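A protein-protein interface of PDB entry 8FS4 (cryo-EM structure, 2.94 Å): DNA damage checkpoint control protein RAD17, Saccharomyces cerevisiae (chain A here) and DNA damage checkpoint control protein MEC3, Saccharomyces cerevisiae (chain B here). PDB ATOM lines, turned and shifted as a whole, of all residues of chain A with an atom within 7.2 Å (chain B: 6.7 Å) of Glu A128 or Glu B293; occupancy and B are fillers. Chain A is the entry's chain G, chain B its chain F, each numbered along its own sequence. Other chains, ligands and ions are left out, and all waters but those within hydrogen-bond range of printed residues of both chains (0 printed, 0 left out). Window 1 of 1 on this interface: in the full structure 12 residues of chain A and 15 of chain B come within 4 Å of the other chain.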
ATOM      1  N   SER A  92     -24.042 -19.743 -32.201  1.00  0.00           N
ATOM      2  CA  SER A  92     -23.944 -18.653 -31.238  1.00  0.00           C
ATOM      3  C   SER A  92     -22.878 -18.952 -30.190  1.00  0.00           C
ATOM      4  O   SER A  92     -21.903 -18.202 -30.037  1.00  0.00           O
ATOM      5  CB  SER A  92     -25.304 -18.417 -30.580  1.00  0.00           C
ATOM      6  OG  SER A  92     -25.580 -19.410 -29.610  1.00  0.00           O
ATOM      7  N   VAL A  95     -19.042 -18.672 -31.047  1.00  0.00           N
ATOM      8  CA  VAL A  95     -18.379 -17.373 -30.988  1.00  0.00           C
ATOM      9  C   VAL A  95     -18.459 -16.767 -29.595  1.00  0.00           C
ATOM     10  O   VAL A  95     -17.665 -15.875 -29.271  1.00  0.00           O
ATOM     11  CB  VAL A  95     -18.952 -16.374 -32.013  1.00  0.00           C
ATOM     12  CG1 VAL A  95     -18.243 -16.523 -33.351  1.00  0.00           C
ATOM     13  CG2 VAL A  95     -20.459 -16.533 -32.180  1.00  0.00           C
ATOM     14  N   MET A  96     -19.394 -17.221 -28.758  1.00  0.00           N
ATOM     15  CA  MET A  96     -19.424 -16.724 -27.383  1.00  0.00           C
ATOM     16  C   MET A  96     -18.302 -17.321 -26.544  1.00  0.00           C
ATOM     17  O   MET A  96     -17.827 -16.677 -25.601  1.00  0.00           O
ATOM     18  CB  MET A  96     -20.771 -17.021 -26.734  1.00  0.00           C
ATOM     19  CG  MET A  96     -21.931 -16.683 -27.619  1.00  0.00           C
ATOM     20  SD  MET A  96     -23.227 -15.796 -26.772  1.00  0.00           S
ATOM     21  CE  MET A  96     -24.206 -15.366 -28.193  1.00  0.00           C
ATOM     22  N   ASN A  99     -13.983 -15.930 -25.523  1.00  0.00           N
ATOM     23  CA  ASN A  99     -13.353 -15.459 -24.294  1.00  0.00           C
ATOM     24  C   ASN A  99     -13.918 -16.214 -23.097  1.00  0.00           C
ATOM     25  O   ASN A  99     -14.241 -15.613 -22.067  1.00  0.00           O
ATOM     26  CB  ASN A  99     -13.555 -13.951 -24.126  1.00  0.00           C
ATOM     27  CG  ASN A  99     -14.972 -13.511 -24.436  1.00  0.00           C
ATOM     28  OD1 ASN A  99     -15.866 -14.338 -24.614  1.00  0.00           O
ATOM     29  ND2 ASN A  99     -15.182 -12.201 -24.504  1.00  0.00           N
ATOM     30  N   VAL A 118     -34.162 -17.490 -24.135  1.00  0.00           N
ATOM     31  CA  VAL A 118     -33.149 -16.472 -23.882  1.00  0.00           C
ATOM     32  C   VAL A 118     -31.921 -17.130 -23.272  1.00  0.00           C
ATOM     33  O   VAL A 118     -32.034 -18.077 -22.485  1.00  0.00           O
ATOM     34  CB  VAL A 118     -33.689 -15.359 -22.965  1.00  0.00           C
ATOM     35  CG1 VAL A 118     -32.863 -14.091 -23.132  1.00  0.00           C
ATOM     36  CG2 VAL A 118     -35.166 -15.088 -23.246  1.00  0.00           C
ATOM     37  N   LEU A 119     -30.742 -16.625 -23.637  1.00  0.00           N
ATOM     38  CA  LEU A 119     -29.462 -17.160 -23.161  1.00  0.00           C
ATOM     39  C   LEU A 119     -28.512 -15.979 -22.972  1.00  0.00           C
ATOM     40  O   LEU A 119     -27.829 -15.563 -23.913  1.00  0.00           O
ATOM     41  CB  LEU A 119     -28.909 -18.183 -24.145  1.00  0.00           C
ATOM     42  CG  LEU A 119     -27.660 -18.947 -23.717  1.00  0.00           C
ATOM     43  CD1 LEU A 119     -27.913 -20.442 -23.793  1.00  0.00           C
ATOM     44  CD2 LEU A 119     -26.476 -18.554 -24.584  1.00  0.00           C
ATOM     45  N   ILE A 120     -28.458 -15.453 -21.749  1.00  0.00           N
ATOM     46  CA  ILE A 120     -27.723 -14.228 -21.447  1.00  0.00           C
ATOM     47  C   ILE A 120     -26.346 -14.590 -20.914  1.00  0.00           C
ATOM     48  O   ILE A 120     -26.219 -15.439 -20.023  1.00  0.00           O
ATOM     49  CB  ILE A 120     -28.484 -13.354 -20.435  1.00  0.00           C
ATOM     50  CG1 ILE A 120     -29.962 -13.240 -20.818  1.00  0.00           C
ATOM     51  CG2 ILE A 120     -27.864 -11.973 -20.368  1.00  0.00           C
ATOM     52  CD1 ILE A 120     -30.900 -13.922 -19.848  1.00  0.00           C
ATOM     53  N   PHE A 121     -25.316 -13.941 -21.453  1.00  0.00           N
ATOM     54  CA  PHE A 121     -23.931 -14.135 -21.031  1.00  0.00           C
ATOM     55  C   PHE A 121     -23.417 -12.816 -20.471  1.00  0.00           C
ATOM     56  O   PHE A 121     -23.150 -11.879 -21.231  1.00  0.00           O
ATOM     57  CB  PHE A 121     -23.063 -14.598 -22.202  1.00  0.00           C
ATOM     58  CG  PHE A 121     -23.044 -16.087 -22.402  1.00  0.00           C
ATOM     59  CD1 PHE A 121     -24.054 -16.890 -21.898  1.00  0.00           C
ATOM     60  CD2 PHE A 121     -22.014 -16.683 -23.108  1.00  0.00           C
ATOM     61  CE1 PHE A 121     -24.030 -18.258 -22.089  1.00  0.00           C
ATOM     62  CE2 PHE A 121     -21.986 -18.050 -23.302  1.00  0.00           C
ATOM     63  CZ  PHE A 121     -22.996 -18.838 -22.792  1.00  0.00           C
ATOM     64  N   GLU A 122     -23.268 -12.742 -19.151  1.00  0.00           N
ATOM     65  CA  GLU A 122     -22.807 -11.534 -18.478  1.00  0.00           C
ATOM     66  C   GLU A 122     -21.398 -11.750 -17.945  1.00  0.00           C
ATOM     67  O   GLU A 122     -21.135 -12.737 -17.252  1.00  0.00           O
ATOM     68  CB  GLU A 122     -23.745 -11.135 -17.334  1.00  0.00           C
ATOM     69  CG  GLU A 122     -24.302 -12.289 -16.517  1.00  0.00           C
ATOM     70  CD  GLU A 122     -25.759 -12.568 -16.826  1.00  0.00           C
ATOM     71  OE1 GLU A 122     -26.064 -12.921 -17.984  1.00  0.00           O
ATOM     72  OE2 GLU A 122     -26.600 -12.432 -15.913  1.00  0.00           O
ATOM     73  N   ASP A 123     -20.497 -10.823 -18.273  1.00  0.00           N
ATOM     74  CA  ASP A 123     -19.118 -10.853 -17.804  1.00  0.00           C
ATOM     75  C   ASP A 123     -18.839  -9.756 -16.784  1.00  0.00           C
ATOM     76  O   ASP A 123     -17.675  -9.429 -16.531  1.00  0.00           O
ATOM     77  CB  ASP A 123     -18.157 -10.727 -18.987  1.00  0.00           C
ATOM     78  CG  ASP A 123     -18.414 -11.765 -20.059  1.00  0.00           C
ATOM     79  OD1 ASP A 123     -19.308 -12.613 -19.860  1.00  0.00           O
ATOM     80  OD2 ASP A 123     -17.725 -11.730 -21.099  1.00  0.00           O
ATOM     81  N   ILE A 126     -20.055  -6.815 -20.010  1.00  0.00           N
ATOM     82  CA  ILE A 126     -20.861  -7.001 -21.214  1.00  0.00           C
ATOM     83  C   ILE A 126     -21.913  -8.055 -20.907  1.00  0.00           C
ATOM     84  O   ILE A 126     -21.595  -9.107 -20.343  1.00  0.00           O
ATOM     85  CB  ILE A 126     -20.019  -7.434 -22.432  1.00  0.00           C
ATOM     86  CG1 ILE A 126     -18.806  -6.525 -22.670  1.00  0.00           C
ATOM     87  CG2 ILE A 126     -20.877  -7.454 -23.688  1.00  0.00           C
ATOM     88  CD1 ILE A 126     -17.656  -6.710 -21.715  1.00  0.00           C
ATOM     89  N   SER A 127     -23.159  -7.775 -21.277  1.00  0.00           N
ATOM     90  CA  SER A 127     -24.273  -8.696 -21.066  1.00  0.00           C
ATOM     91  C   SER A 127     -24.867  -9.047 -22.426  1.00  0.00           C
ATOM     92  O   SER A 127     -25.843  -8.435 -22.866  1.00  0.00           O
ATOM     93  CB  SER A 127     -25.318  -8.082 -20.143  1.00  0.00           C
ATOM     94  OG  SER A 127     -26.595  -8.647 -20.376  1.00  0.00           O
ATOM     95  N   GLU A 128     -24.284 -10.044 -23.086  1.00  0.00           N
ATOM     96  CA  GLU A 128     -24.817 -10.503 -24.361  1.00  0.00           C
ATOM     97  C   GLU A 128     -26.116 -11.260 -24.126  1.00  0.00           C
ATOM     98  O   GLU A 128     -26.189 -12.133 -23.258  1.00  0.00           O
ATOM     99  CB  GLU A 128     -23.806 -11.399 -25.073  1.00  0.00           C
ATOM    100  CG  GLU A 128     -22.394 -10.833 -25.116  1.00  0.00           C
ATOM    101  CD  GLU A 128     -21.666 -11.145 -26.413  1.00  0.00           C
ATOM    102  OE1 GLU A 128     -22.248 -11.826 -27.283  1.00  0.00           O
ATOM    103  OE2 GLU A 128     -20.506 -10.708 -26.562  1.00  0.00           O
ATOM    104  N   ARG A 129     -27.143 -10.921 -24.898  1.00  0.00           N
ATOM    105  CA  ARG A 129     -28.458 -11.531 -24.779  1.00  0.00           C
ATOM    106  C   ARG A 129     -28.869 -12.082 -26.135  1.00  0.00           C
ATOM    107  O   ARG A 129     -28.818 -11.364 -27.139  1.00  0.00           O
ATOM    108  CB  ARG A 129     -29.488 -10.515 -24.279  1.00  0.00           C
ATOM    109  CG  ARG A 129     -30.908 -11.041 -24.204  1.00  0.00           C
ATOM    110  CD  ARG A 129     -31.878  -9.936 -23.837  1.00  0.00           C
ATOM    111  NE  ARG A 129     -33.267 -10.360 -23.979  1.00  0.00           N
ATOM    112  CZ  ARG A 129     -34.044 -10.760 -22.980  1.00  0.00           C
ATOM    113  NH1 ARG A 129     -33.601 -10.818 -21.735  1.00  0.00           N
ATOM    114  NH2 ARG A 129     -35.301 -11.108 -23.237  1.00  0.00           N
ATOM    115  N   VAL A 130     -29.278 -13.347 -26.161  1.00  0.00           N
ATOM    116  CA  VAL A 130     -29.720 -14.007 -27.383  1.00  0.00           C
ATOM    117  C   VAL A 130     -31.094 -14.602 -27.139  1.00  0.00           C
ATOM    118  O   VAL A 130     -31.323 -15.244 -26.109  1.00  0.00           O
ATOM    119  CB  VAL A 130     -28.742 -15.104 -27.835  1.00  0.00           C
ATOM    120  CG1 VAL A 130     -29.254 -15.796 -29.086  1.00  0.00           C
ATOM    121  CG2 VAL A 130     -27.403 -14.511 -28.104  1.00  0.00           C
ATOM    122  N   GLU A 131     -31.999 -14.397 -28.089  1.00  0.00           N
ATOM    123  CA  GLU A 131     -33.346 -14.950 -28.042  1.00  0.00           C
ATOM    124  C   GLU A 131     -33.474 -15.939 -29.193  1.00  0.00           C
ATOM    125  O   GLU A 131     -33.461 -15.542 -30.362  1.00  0.00           O
ATOM    126  CB  GLU A 131     -34.394 -13.845 -28.140  1.00  0.00           C
ATOM    127  CG  GLU A 131     -34.072 -12.589 -27.338  1.00  0.00           C
ATOM    128  CD  GLU A 131     -34.906 -11.396 -27.761  1.00  0.00           C
ATOM    129  OE1 GLU A 131     -34.631 -10.276 -27.281  1.00  0.00           O
ATOM    130  OE2 GLU A 131     -35.837 -11.575 -28.575  1.00  0.00           O
ATOM    131  N   ARG B 252     -16.696  -5.956 -30.076  1.00  0.00           N
ATOM    132  CA  ARG B 252     -17.359  -7.255 -30.033  1.00  0.00           C
ATOM    133  C   ARG B 252     -18.222  -7.498 -31.265  1.00  0.00           C
ATOM    134  O   ARG B 252     -18.471  -8.653 -31.625  1.00  0.00           O
ATOM    135  CB  ARG B 252     -18.210  -7.357 -28.767  1.00  0.00           C
ATOM    136  CG  ARG B 252     -18.783  -8.745 -28.498  1.00  0.00           C
ATOM    137  CD  ARG B 252     -17.748  -9.704 -27.916  1.00  0.00           C
ATOM    138  NE  ARG B 252     -17.027  -9.135 -26.780  1.00  0.00           N
ATOM    139  CZ  ARG B 252     -15.758  -8.745 -26.801  1.00  0.00           C
ATOM    140  NH1 ARG B 252     -15.014  -8.845 -27.893  1.00  0.00           N
ATOM    141  NH2 ARG B 252     -15.219  -8.240 -25.695  1.00  0.00           N
ATOM    142  N   ARG B 255     -16.650  -9.672 -34.625  1.00  0.00           N
ATOM    143  CA  ARG B 255     -16.329 -11.092 -34.696  1.00  0.00           C
ATOM    144  C   ARG B 255     -17.319 -11.882 -35.540  1.00  0.00           C
ATOM    145  O   ARG B 255     -17.126 -13.088 -35.725  1.00  0.00           O
ATOM    146  CB  ARG B 255     -16.257 -11.693 -33.287  1.00  0.00           C
ATOM    147  CG  ARG B 255     -17.560 -11.643 -32.510  1.00  0.00           C
ATOM    148  CD  ARG B 255     -17.437 -12.348 -31.166  1.00  0.00           C
ATOM    149  NE  ARG B 255     -16.282 -11.888 -30.403  1.00  0.00           N
ATOM    150  CZ  ARG B 255     -15.943 -12.347 -29.206  1.00  0.00           C
ATOM    151  NH1 ARG B 255     -16.653 -13.281 -28.595  1.00  0.00           N
ATOM    152  NH2 ARG B 255     -14.861 -11.857 -28.606  1.00  0.00           N
ATOM    153  N   TYR B 256     -18.368 -11.242 -36.051  1.00  0.00           N
ATOM    154  CA  TYR B 256     -19.319 -11.870 -36.962  1.00  0.00           C
ATOM    155  C   TYR B 256     -19.137 -11.229 -38.333  1.00  0.00           C
ATOM    156  O   TYR B 256     -19.417 -10.039 -38.509  1.00  0.00           O
ATOM    157  CB  TYR B 256     -20.752 -11.709 -36.458  1.00  0.00           C
ATOM    158  CG  TYR B 256     -20.891 -11.765 -34.953  1.00  0.00           C
ATOM    159  CD1 TYR B 256     -20.723 -12.956 -34.263  1.00  0.00           C
ATOM    160  CD2 TYR B 256     -21.196 -10.624 -34.223  1.00  0.00           C
ATOM    161  CE1 TYR B 256     -20.853 -13.009 -32.887  1.00  0.00           C
ATOM    162  CE2 TYR B 256     -21.327 -10.668 -32.849  1.00  0.00           C
ATOM    163  CZ  TYR B 256     -21.154 -11.863 -32.186  1.00  0.00           C
ATOM    164  OH  TYR B 256     -21.283 -11.911 -30.817  1.00  0.00           O
ATOM    165  N   LYS B 282     -26.787   0.062 -25.524  1.00  0.00           N
ATOM    166  CA  LYS B 282     -27.013  -1.290 -26.008  1.00  0.00           C
ATOM    167  C   LYS B 282     -26.819  -1.340 -27.516  1.00  0.00           C
ATOM    168  O   LYS B 282     -27.130  -0.384 -28.232  1.00  0.00           O
ATOM    169  CB  LYS B 282     -28.430  -1.763 -25.633  1.00  0.00           C
ATOM    170  CG  LYS B 282     -28.820  -3.135 -26.154  1.00  0.00           C
ATOM    171  CD  LYS B 282     -30.318  -3.368 -26.001  1.00  0.00           C
ATOM    172  CE  LYS B 282     -30.724  -3.482 -24.541  1.00  0.00           C
ATOM    173  NZ  LYS B 282     -31.192  -2.183 -23.986  1.00  0.00           N
ATOM    174  N   ILE B 283     -26.295  -2.468 -27.991  1.00  0.00           N
ATOM    175  CA  ILE B 283     -26.126  -2.737 -29.414  1.00  0.00           C
ATOM    176  C   ILE B 283     -26.961  -3.961 -29.753  1.00  0.00           C
ATOM    177  O   ILE B 283     -26.855  -4.995 -29.082  1.00  0.00           O
ATOM    178  CB  ILE B 283     -24.647  -2.963 -29.782  1.00  0.00           C
ATOM    179  CG1 ILE B 283     -23.853  -1.668 -29.602  1.00  0.00           C
ATOM    180  CG2 ILE B 283     -24.522  -3.474 -31.215  1.00  0.00           C
ATOM    181  CD1 ILE B 283     -22.362  -1.818 -29.819  1.00  0.00           C
ATOM    182  N   ILE B 284     -27.785  -3.847 -30.791  1.00  0.00           N
ATOM    183  CA  ILE B 284     -28.690  -4.912 -31.207  1.00  0.00           C
ATOM    184  C   ILE B 284     -28.351  -5.299 -32.638  1.00  0.00           C
ATOM    185  O   ILE B 284     -28.091  -4.429 -33.477  1.00  0.00           O
ATOM    186  CB  ILE B 284     -30.164  -4.481 -31.090  1.00  0.00           C
ATOM    187  CG1 ILE B 284     -30.430  -3.915 -29.692  1.00  0.00           C
ATOM    188  CG2 ILE B 284     -31.086  -5.652 -31.411  1.00  0.00           C
ATOM    189  CD1 ILE B 284     -31.863  -3.484 -29.446  1.00  0.00           C
ATOM    190  N   VAL B 285     -28.344  -6.600 -32.907  1.00  0.00           N
ATOM    191  CA  VAL B 285     -28.084  -7.145 -34.233  1.00  0.00           C
ATOM    192  C   VAL B 285     -29.292  -7.976 -34.641  1.00  0.00           C
ATOM    193  O   VAL B 285     -29.705  -8.880 -33.905  1.00  0.00           O
ATOM    194  CB  VAL B 285     -26.798  -7.990 -34.250  1.00  0.00           C
ATOM    195  CG1 VAL B 285     -26.709  -8.814 -35.520  1.00  0.00           C
ATOM    196  CG2 VAL B 285     -25.583  -7.092 -34.105  1.00  0.00           C
ATOM    197  N   HIS B 291     -31.586 -13.515 -32.539  1.00  0.00           N
ATOM    198  CA  HIS B 291     -31.657 -12.109 -32.157  1.00  0.00           C
ATOM    199  C   HIS B 291     -30.601 -11.832 -31.095  1.00  0.00           C
ATOM    200  O   HIS B 291     -30.741 -12.258 -29.945  1.00  0.00           O
ATOM    201  CB  HIS B 291     -33.051 -11.760 -31.642  1.00  0.00           C
ATOM    202  CG  HIS B 291     -33.226 -10.310 -31.316  1.00  0.00           C
ATOM    203  ND1 HIS B 291     -33.787  -9.411 -32.197  1.00  0.00           N
ATOM    204  CD2 HIS B 291     -32.912  -9.602 -30.206  1.00  0.00           C
ATOM    205  CE1 HIS B 291     -33.811  -8.212 -31.644  1.00  0.00           C
ATOM    206  NE2 HIS B 291     -33.287  -8.300 -30.435  1.00  0.00           N
ATOM    207  N   LEU B 292     -29.555 -11.105 -31.473  1.00  0.00           N
ATOM    208  CA  LEU B 292     -28.429 -10.819 -30.595  1.00  0.00           C
ATOM    209  C   LEU B 292     -28.518  -9.382 -30.103  1.00  0.00           C
ATOM    210  O   LEU B 292     -28.766  -8.466 -30.893  1.00  0.00           O
ATOM    211  CB  LEU B 292     -27.103 -11.052 -31.326  1.00  0.00           C
ATOM    212  CG  LEU B 292     -25.823 -10.701 -30.567  1.00  0.00           C
ATOM    213  CD1 LEU B 292     -25.719 -11.501 -29.279  1.00  0.00           C
ATOM    214  CD2 LEU B 292     -24.605 -10.943 -31.445  1.00  0.00           C
ATOM    215  N   GLU B 293     -28.332  -9.193 -28.797  1.00  0.00           N
ATOM    216  CA  GLU B 293     -28.299  -7.869 -28.179  1.00  0.00           C
ATOM    217  C   GLU B 293     -27.026  -7.765 -27.353  1.00  0.00           C
ATOM    218  O   GLU B 293     -26.907  -8.411 -26.307  1.00  0.00           O
ATOM    219  CB  GLU B 293     -29.527  -7.630 -27.302  1.00  0.00           C
ATOM    220  CG  GLU B 293     -30.849  -7.767 -28.026  1.00  0.00           C
ATOM    221  CD  GLU B 293     -32.032  -7.431 -27.141  1.00  0.00           C
ATOM    222  OE1 GLU B 293     -31.818  -6.859 -26.052  1.00  0.00           O
ATOM    223  OE2 GLU B 293     -33.177  -7.739 -27.535  1.00  0.00           O
ATOM    224  N   ILE B 294     -26.080  -6.954 -27.811  1.00  0.00           N
ATOM    225  CA  ILE B 294     -24.833  -6.731 -27.091  1.00  0.00           C
ATOM    226  C   ILE B 294     -25.031  -5.505 -26.207  1.00  0.00           C
ATOM    227  O   ILE B 294     -25.117  -4.379 -26.702  1.00  0.00           O
ATOM    228  CB  ILE B 294     -23.655  -6.547 -28.054  1.00  0.00           C
ATOM    229  CG1 ILE B 294     -23.652  -7.661 -29.102  1.00  0.00           C
ATOM    230  CG2 ILE B 294     -22.340  -6.540 -27.294  1.00  0.00           C
ATOM    231  CD1 ILE B 294     -24.185  -7.229 -30.449  1.00  0.00           C
ATOM    232  N   CYS B 295     -25.109  -5.724 -24.899  1.00  0.00           N
ATOM    233  CA  CYS B 295     -25.385  -4.669 -23.935  1.00  0.00           C
ATOM    234  C   CYS B 295     -24.123  -4.315 -23.160  1.00  0.00           C
ATOM    235  O   CYS B 295     -23.089  -4.978 -23.265  1.00  0.00           O
ATOM    236  CB  CYS B 295     -26.499  -5.095 -22.971  1.00  0.00           C
ATOM    237  SG  CYS B 295     -27.786  -6.115 -23.725  1.00  0.00           S
ATOM    238  N   ASN B 297     -23.396  -3.189 -19.166  1.00  0.00           N
ATOM    239  CA  ASN B 297     -23.886  -2.954 -17.815  1.00  0.00           C
ATOM    240  C   ASN B 297     -22.910  -2.155 -16.961  1.00  0.00           C
ATOM    241  O   ASN B 297     -23.181  -1.939 -15.776  1.00  0.00           O
ATOM    242  CB  ASN B 297     -24.199  -4.287 -17.124  1.00  0.00           C
ATOM    243  CG  ASN B 297     -23.111  -5.323 -17.331  1.00  0.00           C
ATOM    244  OD1 ASN B 297     -22.006  -5.194 -16.804  1.00  0.00           O
ATOM    245  ND2 ASN B 297     -23.421  -6.359 -18.100  1.00  0.00           N
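Of the 16 printed residues of chain A, 7 touch a printed residue of chain B. Hydrophobic or aromatic side chains of chain A within 4 Å of the printed part of chain B: Val A95, Ile A126 and Val A130. Of the 13 printed residues of chain B, 9 touch a printed residue of chain A. Among the printed residues, 18 pairs touch across the chains. Among the printed residues, Asp or Glu carboxylates within 4 Å of a Lys or Arg side-chain nitrogen of the other chain: Glu A128 with Arg B252.
Of the printed residues of chain B, Glu A128 touches Arg B252 (3.2 Å), Tyr B256 (3.7 Å) and Glu B293 (3.5 Å). Glu B293 touches just these residues of chain A: Ser A127, Glu A128, Arg A129 and Glu A131. Of the printed residues of chain A, His B291 touches Arg A129, Val A130 and Glu A131. Of the printed residues of chain A, Tyr B256 touches Val A95 and Glu A128. Printed residues of chain A within 4 Å of Arg B255: Val A95 (2.9 Å). Ile A120 touches none of the printed residues of chain B. The nearest printed residue of chain B that does not touch Glu A128 is Leu B292 (4.02 Å).
N of Glu B293 is in hydrogen-bond range of O of Arg A129 (2.8 Å). O of His B291 sits at hydrogen-bond distance from N of Glu A131 (3.1 Å). The guanidinium group (NE) of Arg B252 lies within salt-bridge range of the side-chain carboxylate (OE2) of Glu A128, at 3.8 Å. OE2 of Glu B293 lies close to OE1 of Glu A131, 2.9 Å away. ND2 of Asn B297 lies close to N of Ser A127 (3.5 Å). The backbone carbonyl oxygen (O) of Ser A127 lies within hydrogen-bond range of the side-chain sulfur (SG) of Cys B295, 3.1 Å away. The guanidinium group of Arg B255 sits at hydrogen-bond distance from the backbone carbonyl oxygen of Val A95 (2.9 Å).
NE of Arg A129 lies within salt-bridge range of OE1 of Glu A131 (3.6 Å). The backbone NH (N) of Val B285 sits at hydrogen-bond distance from the backbone carbonyl oxygen (O) of Leu B292, at 2.8 Å. A ring nitrogen (NE2) of His B291 sits at hydrogen-bond distance from the side-chain carboxylate of Glu B293, at 3.0 Å. The backbone NH (N) of Phe A121 lies within hydrogen-bond range of the backbone carbonyl oxygen (O) of Glu A128 (2.7 Å). O of Val A130 lies within hydrogen-bond range of N of Leu A119, 2.9 Å away. The backbone carbonyl oxygen (O) of Ile B283 sits at hydrogen-bond distance from the backbone NH (N) of Ile B294, at 2.5 Å.
Tyr B256 touches Val A95. CG2 of Ile A126 touches CG2 of Ile B294, at 3.997 Å. Cys B295 touches Ile A126. Asn B297 touches Ile A126. O of Ser A127 touches O of Glu B293, 3.6 Å away. Glu A128 touches Glu B293. Arg A129 touches His B291. Arg A129 touches Leu B292 (O to CA, 3.5 Å). CA of Val A130 touches O of His B291, 3.3 Å away. Leu B292 touches Val A130.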
